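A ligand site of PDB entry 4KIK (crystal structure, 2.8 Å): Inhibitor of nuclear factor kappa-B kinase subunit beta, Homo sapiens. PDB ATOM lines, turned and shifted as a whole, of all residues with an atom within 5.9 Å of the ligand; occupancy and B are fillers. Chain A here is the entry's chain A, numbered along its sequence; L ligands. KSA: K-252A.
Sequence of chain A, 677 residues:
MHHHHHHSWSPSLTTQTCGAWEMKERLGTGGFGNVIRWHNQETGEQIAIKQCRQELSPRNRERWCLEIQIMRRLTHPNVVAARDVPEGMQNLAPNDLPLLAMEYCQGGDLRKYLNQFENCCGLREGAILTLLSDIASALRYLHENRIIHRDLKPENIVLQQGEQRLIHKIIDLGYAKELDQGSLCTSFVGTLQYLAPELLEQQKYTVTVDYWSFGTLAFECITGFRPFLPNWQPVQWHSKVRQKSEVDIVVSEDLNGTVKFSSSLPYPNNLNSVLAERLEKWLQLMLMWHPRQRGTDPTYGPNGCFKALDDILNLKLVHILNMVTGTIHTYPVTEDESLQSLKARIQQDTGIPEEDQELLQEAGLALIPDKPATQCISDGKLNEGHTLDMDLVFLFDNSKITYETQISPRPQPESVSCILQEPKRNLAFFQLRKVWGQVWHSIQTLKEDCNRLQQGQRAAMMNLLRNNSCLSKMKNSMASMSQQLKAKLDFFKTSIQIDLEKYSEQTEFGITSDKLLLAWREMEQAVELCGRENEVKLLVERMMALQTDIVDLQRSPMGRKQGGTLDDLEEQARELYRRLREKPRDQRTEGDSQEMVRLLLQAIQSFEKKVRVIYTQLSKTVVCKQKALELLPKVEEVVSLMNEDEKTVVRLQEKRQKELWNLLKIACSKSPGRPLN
The backbone carbonyl oxygen (O) of Glu 155 is in hydrogen-bond range of an oxygen (O4) of the ligand (2.7 Å).
The backbone NH of Cys 105 sits at hydrogen-bond distance from an oxygen (O2) of the ligand.
A nitrogen (N3) of the ligand lies within hydrogen-bond range of the backbone carbonyl oxygen (O) of Glu 103 (3.0 Å).
O of Ala 48 lies within hydrogen-bond range of N of Met 102, at 2.8 Å.
The backbone carbonyl oxygen (O) of Val 35 lies within hydrogen-bond range of the backbone NH (N) of Leu 27, 2.8 Å away.
The backbone carbonyl oxygen (O) of Gly 28 lies within hydrogen-bond range of the backbone NH (N) of Val 35.
O of Asn 156 lies within hydrogen-bond range of N of Ile 171 (3.0 Å).
OD1 of Asp 172 is in salt-bridge range of NZ of Lys 50, at 3.6 Å.
NZ of Lys 50 is in salt-bridge range of OE2 of Glu 67, at 3.0 Å.
The backbone NH of Lys 50 is in hydrogen-bond range of the backbone carbonyl oxygen of Leu 100, at 2.9 Å.
Leu 27 touches the ligand.
Gly 28 touches the ligand.
Thr 29 touches the ligand.
Val 35 touches the ligand (CG2 to C10, 3.7 Å).
CB of Ala 48 touches N3 of the ligand (3.4 Å).
Lys 50 touches the ligand (CD to C13, 3.7 Å).
Met 102 touches the ligand (SD to C14, 3.7 Å).
Tyr 104 touches the ligand.
CA of Gly 108 touches C19 of the ligand, at 3.5 Å.
Asp 109 touches the ligand (OD2 to C18, 3.8 Å).
OD1 of Asn 156 touches O4 of the ligand, 3.8 Å away.
CG1 of Val 158 touches C5 of the ligand, 3.8 Å away.
CD1 of Ile 171 touches O4 of the ligand, at 3.4 Å.
OD1 of Asp 172 touches C12 of the ligand (3.7 Å).
Of the 26 residues printed, 17 come within 4 Å of the ligand.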
ATOM      1  N   LEU A  27     -21.375   7.641 -32.372  1.00  0.00           N
ATOM      2  CA  LEU A  27     -22.127   8.883 -32.327  1.00  0.00           C
ATOM      3  C   LEU A  27     -21.528   9.875 -31.277  1.00  0.00           C
ATOM      4  O   LEU A  27     -21.596  11.091 -31.459  1.00  0.00           O
ATOM      5  CB  LEU A  27     -23.624   8.578 -32.074  1.00  0.00           C
ATOM      6  CG  LEU A  27     -24.282   7.638 -33.086  1.00  0.00           C
ATOM      7  CD1 LEU A  27     -25.668   7.234 -32.645  1.00  0.00           C
ATOM      8  CD2 LEU A  27     -24.273   8.222 -34.473  1.00  0.00           C
ATOM      9  N   GLY A  28     -20.894   9.331 -30.253  1.00  0.00           N
ATOM     10  CA  GLY A  28     -20.266  10.078 -29.180  1.00  0.00           C
ATOM     11  C   GLY A  28     -19.973   9.164 -28.008  1.00  0.00           C
ATOM     12  O   GLY A  28     -20.400   8.007 -27.993  1.00  0.00           O
ATOM     13  N   THR A  29     -19.267   9.707 -26.981  1.00  0.00           N
ATOM     14  CA  THR A  29     -18.832   8.944 -25.804  1.00  0.00           C
ATOM     15  C   THR A  29     -19.435   9.532 -24.495  1.00  0.00           C
ATOM     16  O   THR A  29     -19.311  10.717 -24.207  1.00  0.00           O
ATOM     17  CB  THR A  29     -17.295   8.807 -25.773  1.00  0.00           C
ATOM     18  OG1 THR A  29     -16.884   8.312 -24.507  1.00  0.00           O
ATOM     19  CG2 THR A  29     -16.555  10.110 -26.092  1.00  0.00           C
ATOM     20  N   GLY A  33     -20.248   4.656 -20.902  1.00  0.00           N
ATOM     21  CA  GLY A  33     -19.774   4.108 -22.177  1.00  0.00           C
ATOM     22  C   GLY A  33     -20.232   4.811 -23.453  1.00  0.00           C
ATOM     23  O   GLY A  33     -20.936   5.822 -23.402  1.00  0.00           O
ATOM     24  N   VAL A  35     -21.877   5.403 -27.483  1.00  0.00           N
ATOM     25  CA  VAL A  35     -23.098   5.352 -28.288  1.00  0.00           C
ATOM     26  C   VAL A  35     -22.659   5.130 -29.768  1.00  0.00           C
ATOM     27  O   VAL A  35     -21.848   5.895 -30.298  1.00  0.00           O
ATOM     28  CB  VAL A  35     -23.982   6.596 -28.098  1.00  0.00           C
ATOM     29  CG1 VAL A  35     -25.273   6.472 -28.886  1.00  0.00           C
ATOM     30  CG2 VAL A  35     -24.283   6.812 -26.628  1.00  0.00           C
ATOM     31  N   ALA A  48     -29.579   3.625 -32.277  1.00  0.00           N
ATOM     32  CA  ALA A  48     -28.406   4.072 -31.499  1.00  0.00           C
ATOM     33  C   ALA A  48     -28.244   3.137 -30.286  1.00  0.00           C
ATOM     34  O   ALA A  48     -29.232   2.891 -29.582  1.00  0.00           O
ATOM     35  CB  ALA A  48     -28.568   5.512 -31.052  1.00  0.00           C
ATOM     36  N   LYS A  50     -26.387   2.421 -26.681  1.00  0.00           N
ATOM     37  CA  LYS A  50     -25.486   2.791 -25.616  1.00  0.00           C
ATOM     38  C   LYS A  50     -25.013   1.464 -24.987  1.00  0.00           C
ATOM     39  O   LYS A  50     -25.826   0.596 -24.679  1.00  0.00           O
ATOM     40  CB  LYS A  50     -26.127   3.744 -24.617  1.00  0.00           C
ATOM     41  CG  LYS A  50     -25.093   4.470 -23.750  1.00  0.00           C
ATOM     42  CD  LYS A  50     -25.705   5.632 -23.007  1.00  0.00           C
ATOM     43  CE  LYS A  50     -25.390   5.631 -21.524  1.00  0.00           C
ATOM     44  NZ  LYS A  50     -26.153   6.695 -20.800  1.00  0.00           N
ATOM     45  N   GLU A  67     -31.799   3.783 -15.830  1.00  0.00           N
ATOM     46  CA  GLU A  67     -31.940   4.633 -17.019  1.00  0.00           C
ATOM     47  C   GLU A  67     -32.706   3.887 -18.125  1.00  0.00           C
ATOM     48  O   GLU A  67     -33.645   4.460 -18.689  1.00  0.00           O
ATOM     49  CB  GLU A  67     -30.579   5.104 -17.554  1.00  0.00           C
ATOM     50  CG  GLU A  67     -30.714   6.288 -18.493  1.00  0.00           C
ATOM     51  CD  GLU A  67     -29.482   6.622 -19.299  1.00  0.00           C
ATOM     52  OE1 GLU A  67     -29.643   7.151 -20.426  1.00  0.00           O
ATOM     53  OE2 GLU A  67     -28.354   6.342 -18.813  1.00  0.00           O
ATOM     54  N   VAL A  80     -36.089  11.131 -26.876  1.00  0.00           N
ATOM     55  CA  VAL A  80     -35.625   9.964 -27.643  1.00  0.00           C
ATOM     56  C   VAL A  80     -36.318   8.649 -27.160  1.00  0.00           C
ATOM     57  O   VAL A  80     -36.356   8.307 -25.967  1.00  0.00           O
ATOM     58  CB  VAL A  80     -34.073   9.855 -27.681  1.00  0.00           C
ATOM     59  CG1 VAL A  80     -33.558   8.506 -28.141  1.00  0.00           C
ATOM     60  CG2 VAL A  80     -33.550  10.927 -28.607  1.00  0.00           C
ATOM     61  N   LEU A 100     -28.524  -0.387 -24.261  1.00  0.00           N
ATOM     62  CA  LEU A 100     -29.622   0.564 -24.349  1.00  0.00           C
ATOM     63  C   LEU A 100     -29.880   0.886 -25.817  1.00  0.00           C
ATOM     64  O   LEU A 100     -29.113   1.622 -26.421  1.00  0.00           O
ATOM     65  CB  LEU A 100     -29.330   1.828 -23.526  1.00  0.00           C
ATOM     66  CG  LEU A 100     -30.421   2.948 -23.515  1.00  0.00           C
ATOM     67  CD1 LEU A 100     -31.812   2.415 -23.114  1.00  0.00           C
ATOM     68  CD2 LEU A 100     -30.011   4.103 -22.638  1.00  0.00           C
ATOM     69  N   MET A 102     -31.845   2.761 -28.698  1.00  0.00           N
ATOM     70  CA  MET A 102     -32.612   3.993 -28.836  1.00  0.00           C
ATOM     71  C   MET A 102     -32.843   4.361 -30.297  1.00  0.00           C
ATOM     72  O   MET A 102     -32.168   3.813 -31.163  1.00  0.00           O
ATOM     73  CB  MET A 102     -31.902   5.169 -28.140  1.00  0.00           C
ATOM     74  CG  MET A 102     -31.772   5.001 -26.639  1.00  0.00           C
ATOM     75  SD  MET A 102     -30.340   5.894 -25.988  1.00  0.00           S
ATOM     76  CE  MET A 102     -28.989   5.083 -26.837  1.00  0.00           C
ATOM     77  N   GLU A 103     -33.781   5.277 -30.562  1.00  0.00           N
ATOM     78  CA  GLU A 103     -34.055   5.734 -31.912  1.00  0.00           C
ATOM     79  C   GLU A 103     -32.846   6.541 -32.421  1.00  0.00           C
ATOM     80  O   GLU A 103     -32.209   7.229 -31.619  1.00  0.00           O
ATOM     81  CB  GLU A 103     -35.378   6.562 -31.964  1.00  0.00           C
ATOM     82  CG  GLU A 103     -35.282   8.075 -31.860  1.00  0.00           C
ATOM     83  CD  GLU A 103     -36.602   8.825 -32.024  1.00  0.00           C
ATOM     84  OE1 GLU A 103     -37.056   8.970 -33.180  1.00  0.00           O
ATOM     85  OE2 GLU A 103     -37.150   9.277 -30.999  1.00  0.00           O
ATOM     86  N   TYR A 104     -32.515   6.443 -33.736  1.00  0.00           N
ATOM     87  CA  TYR A 104     -31.414   7.254 -34.279  1.00  0.00           C
ATOM     88  C   TYR A 104     -31.967   8.586 -34.799  1.00  0.00           C
ATOM     89  O   TYR A 104     -32.928   8.604 -35.584  1.00  0.00           O
ATOM     90  CB  TYR A 104     -30.649   6.516 -35.373  1.00  0.00           C
ATOM     91  CG  TYR A 104     -29.609   7.366 -36.062  1.00  0.00           C
ATOM     92  CD1 TYR A 104     -29.726   7.697 -37.413  1.00  0.00           C
ATOM     93  CD2 TYR A 104     -28.521   7.877 -35.362  1.00  0.00           C
ATOM     94  CE1 TYR A 104     -28.786   8.508 -38.038  1.00  0.00           C
ATOM     95  CE2 TYR A 104     -27.570   8.698 -35.981  1.00  0.00           C
ATOM     96  CZ  TYR A 104     -27.702   9.001 -37.336  1.00  0.00           C
ATOM     97  OH  TYR A 104     -26.751   9.768 -37.962  1.00  0.00           O
ATOM     98  N   CYS A 105     -31.358   9.708 -34.322  1.00  0.00           N
ATOM     99  CA  CYS A 105     -31.761  11.061 -34.692  1.00  0.00           C
ATOM    100  C   CYS A 105     -30.773  11.621 -35.707  1.00  0.00           C
ATOM    101  O   CYS A 105     -29.668  12.019 -35.349  1.00  0.00           O
ATOM    102  CB  CYS A 105     -31.878  11.928 -33.445  1.00  0.00           C
ATOM    103  SG  CYS A 105     -33.131  11.368 -32.267  1.00  0.00           S
ATOM    104  N   GLN A 106     -31.185  11.592 -36.984  1.00  0.00           N
ATOM    105  CA  GLN A 106     -30.442  11.970 -38.205  1.00  0.00           C
ATOM    106  C   GLN A 106     -29.806  13.364 -38.213  1.00  0.00           C
ATOM    107  O   GLN A 106     -28.830  13.595 -38.893  1.00  0.00           O
ATOM    108  CB  GLN A 106     -31.370  11.847 -39.422  1.00  0.00           C
ATOM    109  CG  GLN A 106     -31.556  10.399 -39.853  1.00  0.00           C
ATOM    110  CD  GLN A 106     -32.843  10.183 -40.615  1.00  0.00           C
ATOM    111  OE1 GLN A 106     -33.813   9.638 -40.080  1.00  0.00           O
ATOM    112  NE2 GLN A 106     -32.882  10.645 -41.842  1.00  0.00           N
ATOM    113  N   GLY A 107     -30.371  14.263 -37.465  1.00  0.00           N
ATOM    114  CA  GLY A 107     -29.901  15.639 -37.395  1.00  0.00           C
ATOM    115  C   GLY A 107     -28.636  15.804 -36.591  1.00  0.00           C
ATOM    116  O   GLY A 107     -27.903  16.758 -36.808  1.00  0.00           O
ATOM    117  N   GLY A 108     -28.368  14.870 -35.694  1.00  0.00           N
ATOM    118  CA  GLY A 108     -27.202  14.964 -34.842  1.00  0.00           C
ATOM    119  C   GLY A 108     -27.469  15.845 -33.629  1.00  0.00           C
ATOM    120  O   GLY A 108     -28.579  16.357 -33.440  1.00  0.00           O
ATOM    121  N   ASP A 109     -26.450  16.020 -32.777  1.00  0.00           N
ATOM    122  CA  ASP A 109     -26.590  16.804 -31.562  1.00  0.00           C
ATOM    123  C   ASP A 109     -26.592  18.345 -31.837  1.00  0.00           C
ATOM    124  O   ASP A 109     -26.158  18.807 -32.897  1.00  0.00           O
ATOM    125  CB  ASP A 109     -25.492  16.404 -30.553  1.00  0.00           C
ATOM    126  CG  ASP A 109     -24.086  16.662 -31.033  1.00  0.00           C
ATOM    127  OD1 ASP A 109     -23.336  17.333 -30.288  1.00  0.00           O
ATOM    128  OD2 ASP A 109     -23.733  16.188 -32.151  1.00  0.00           O
ATOM    129  N   LYS A 112     -23.091  20.248 -32.434  1.00  0.00           N
ATOM    130  CA  LYS A 112     -22.661  20.215 -33.838  1.00  0.00           C
ATOM    131  C   LYS A 112     -23.251  21.400 -34.595  1.00  0.00           C
ATOM    132  O   LYS A 112     -22.525  22.034 -35.342  1.00  0.00           O
ATOM    133  CB  LYS A 112     -23.056  18.877 -34.485  1.00  0.00           C
ATOM    134  CG  LYS A 112     -22.623  18.688 -35.968  1.00  0.00           C
ATOM    135  CD  LYS A 112     -22.792  17.214 -36.475  1.00  0.00           C
ATOM    136  CE  LYS A 112     -23.070  17.046 -37.973  1.00  0.00           C
ATOM    137  NZ  LYS A 112     -23.912  15.831 -38.290  1.00  0.00           N
ATOM    138  N   LYS A 153     -27.980  20.278 -21.669  1.00  0.00           N
ATOM    139  CA  LYS A 153     -26.973  21.032 -22.438  1.00  0.00           C
ATOM    140  C   LYS A 153     -27.052  20.678 -23.916  1.00  0.00           C
ATOM    141  O   LYS A 153     -27.678  19.665 -24.236  1.00  0.00           O
ATOM    142  CB  LYS A 153     -25.546  20.776 -21.876  1.00  0.00           C
ATOM    143  CG  LYS A 153     -25.043  19.367 -22.036  1.00  0.00           C
ATOM    144  CD  LYS A 153     -23.932  19.068 -21.098  1.00  0.00           C
ATOM    145  CE  LYS A 153     -23.550  17.618 -21.257  1.00  0.00           C
ATOM    146  NZ  LYS A 153     -22.391  17.277 -20.385  1.00  0.00           N
ATOM    147  N   GLU A 155     -25.148  19.044 -25.900  1.00  0.00           N
ATOM    148  CA  GLU A 155     -24.656  17.676 -26.086  1.00  0.00           C
ATOM    149  C   GLU A 155     -25.735  16.666 -25.732  1.00  0.00           C
ATOM    150  O   GLU A 155     -25.660  15.506 -26.142  1.00  0.00           O
ATOM    151  CB  GLU A 155     -23.413  17.429 -25.200  1.00  0.00           C
ATOM    152  CG  GLU A 155     -22.186  18.198 -25.649  1.00  0.00           C
ATOM    153  CD  GLU A 155     -21.972  19.619 -25.136  1.00  0.00           C
ATOM    154  OE1 GLU A 155     -22.911  20.210 -24.555  1.00  0.00           O
ATOM    155  OE2 GLU A 155     -20.857  20.142 -25.308  1.00  0.00           O
ATOM    156  N   ASN A 156     -26.743  17.114 -24.960  1.00  0.00           N
ATOM    157  CA  ASN A 156     -27.840  16.258 -24.510  1.00  0.00           C
ATOM    158  C   ASN A 156     -29.155  16.541 -25.264  1.00  0.00           C
ATOM    159  O   ASN A 156     -30.205  16.107 -24.848  1.00  0.00           O
ATOM    160  CB  ASN A 156     -27.994  16.397 -22.999  1.00  0.00           C
ATOM    161  CG  ASN A 156     -26.970  15.576 -22.241  1.00  0.00           C
ATOM    162  OD1 ASN A 156     -26.137  14.889 -22.815  1.00  0.00           O
ATOM    163  ND2 ASN A 156     -27.059  15.565 -20.940  1.00  0.00           N
ATOM    164  N   VAL A 158     -30.555  16.162 -29.268  1.00  0.00           N
ATOM    165  CA  VAL A 158     -30.316  15.606 -30.607  1.00  0.00           C
ATOM    166  C   VAL A 158     -31.504  16.004 -31.500  1.00  0.00           C
ATOM    167  O   VAL A 158     -32.615  16.275 -31.001  1.00  0.00           O
ATOM    168  CB  VAL A 158     -29.985  14.080 -30.656  1.00  0.00           C
ATOM    169  CG1 VAL A 158     -28.562  13.807 -30.149  1.00  0.00           C
ATOM    170  CG2 VAL A 158     -31.006  13.244 -29.897  1.00  0.00           C
ATOM    171  N   ILE A 171     -31.979  13.640 -24.606  1.00  0.00           N
ATOM    172  CA  ILE A 171     -31.261  12.394 -24.364  1.00  0.00           C
ATOM    173  C   ILE A 171     -30.572  12.477 -22.986  1.00  0.00           C
ATOM    174  O   ILE A 171     -30.650  13.497 -22.309  1.00  0.00           O
ATOM    175  CB  ILE A 171     -30.260  12.014 -25.502  1.00  0.00           C
ATOM    176  CG1 ILE A 171     -29.452  13.209 -26.030  1.00  0.00           C
ATOM    177  CG2 ILE A 171     -30.990  11.353 -26.605  1.00  0.00           C
ATOM    178  CD1 ILE A 171     -28.061  12.921 -26.483  1.00  0.00           C
ATOM    179  N   ASP A 172     -29.945  11.360 -22.581  1.00  0.00           N
ATOM    180  CA  ASP A 172     -29.175  11.139 -21.366  1.00  0.00           C
ATOM    181  C   ASP A 172     -29.969  11.448 -20.103  1.00  0.00           C
ATOM    182  O   ASP A 172     -29.788  12.506 -19.479  1.00  0.00           O
ATOM    183  CB  ASP A 172     -27.836  11.903 -21.388  1.00  0.00           C
ATOM    184  CG  ASP A 172     -26.846  11.401 -20.343  1.00  0.00           C
ATOM    185  OD1 ASP A 172     -26.752  10.147 -20.164  1.00  0.00           O
ATOM    186  OD2 ASP A 172     -26.173  12.245 -19.710  1.00  0.00           O
ATOM    187  N   LEU A 173     -30.816  10.487 -19.703  1.00  0.00           N
ATOM    188  CA  LEU A 173     -31.617  10.602 -18.501  1.00  0.00           C
ATOM    189  C   LEU A 173     -30.991   9.702 -17.417  1.00  0.00           C
ATOM    190  O   LEU A 173     -31.720   9.028 -16.658  1.00  0.00           O
ATOM    191  CB  LEU A 173     -33.106  10.279 -18.752  1.00  0.00           C
ATOM    192  CG  LEU A 173     -33.750  10.722 -20.091  1.00  0.00           C
ATOM    193  CD1 LEU A 173     -35.169  10.315 -20.127  1.00  0.00           C
ATOM    194  CD2 LEU A 173     -33.688  12.232 -20.307  1.00  0.00           C
HETATM  195  O3  KSA L   1     -22.184  13.833 -25.420  1.00  0.00           O
HETATM  196  C22 KSA L   1     -22.428  13.318 -26.475  1.00  0.00           C
HETATM  197  O5  KSA L   1     -21.528  13.145 -27.444  1.00  0.00           O
HETATM  198  C26 KSA L   1     -20.138  13.293 -27.061  1.00  0.00           C
HETATM  199  C1  KSA L   1     -23.817  12.764 -26.856  1.00  0.00           C
HETATM  200  O4  KSA L   1     -24.704  12.993 -25.752  1.00  0.00           O
HETATM  201  C2  KSA L   1     -23.891  11.191 -27.132  1.00  0.00           C
HETATM  202  O1  KSA L   1     -23.413  11.146 -28.456  1.00  0.00           O
HETATM  203  C25 KSA L   1     -22.913  10.332 -26.361  1.00  0.00           C
HETATM  204  N1  KSA L   1     -25.316  10.597 -27.100  1.00  0.00           N
HETATM  205  C3  KSA L   1     -26.128  10.392 -28.231  1.00  0.00           C
HETATM  206  C4  KSA L   1     -25.941  10.820 -29.574  1.00  0.00           C
HETATM  207  N2  KSA L   1     -24.977  11.640 -30.093  1.00  0.00           N
HETATM  208  C24 KSA L   1     -23.906  12.228 -29.239  1.00  0.00           C
HETATM  209  C27 KSA L   1     -24.321  13.290 -28.223  1.00  0.00           C
HETATM  210  C17 KSA L   1     -25.207  11.767 -31.473  1.00  0.00           C
HETATM  211  C18 KSA L   1     -24.534  12.524 -32.420  1.00  0.00           C
HETATM  212  C19 KSA L   1     -24.994  12.504 -33.733  1.00  0.00           C
HETATM  213  C20 KSA L   1     -26.091  11.727 -34.092  1.00  0.00           C
HETATM  214  C21 KSA L   1     -26.769  10.982 -33.140  1.00  0.00           C
HETATM  215  C16 KSA L   1     -26.352  11.006 -31.812  1.00  0.00           C
HETATM  216  C5  KSA L   1     -26.846  10.436 -30.594  1.00  0.00           C
HETATM  217  C6  KSA L   1     -27.962   9.669 -30.213  1.00  0.00           C
HETATM  218  C15 KSA L   1     -29.122   9.217 -31.005  1.00  0.00           C
HETATM  219  O2  KSA L   1     -29.377   9.451 -32.191  1.00  0.00           O
HETATM  220  C7  KSA L   1     -28.177   9.247 -28.885  1.00  0.00           C
HETATM  221  C23 KSA L   1     -29.416   8.392 -28.789  1.00  0.00           C
HETATM  222  N3  KSA L   1     -29.957   8.479 -30.163  1.00  0.00           N
HETATM  223  C8  KSA L   1     -27.259   9.624 -27.892  1.00  0.00           C
HETATM  224  C9  KSA L   1     -27.180   9.398 -26.461  1.00  0.00           C
HETATM  225  C10 KSA L   1     -25.990  10.006 -26.003  1.00  0.00           C
HETATM  226  C11 KSA L   1     -25.630   9.954 -24.658  1.00  0.00           C
HETATM  227  C14 KSA L   1     -27.990   8.705 -25.540  1.00  0.00           C
HETATM  228  C13 KSA L   1     -27.605   8.634 -24.207  1.00  0.00           C
HETATM  229  C12 KSA L   1     -26.440   9.257 -23.765  1.00  0.00           C
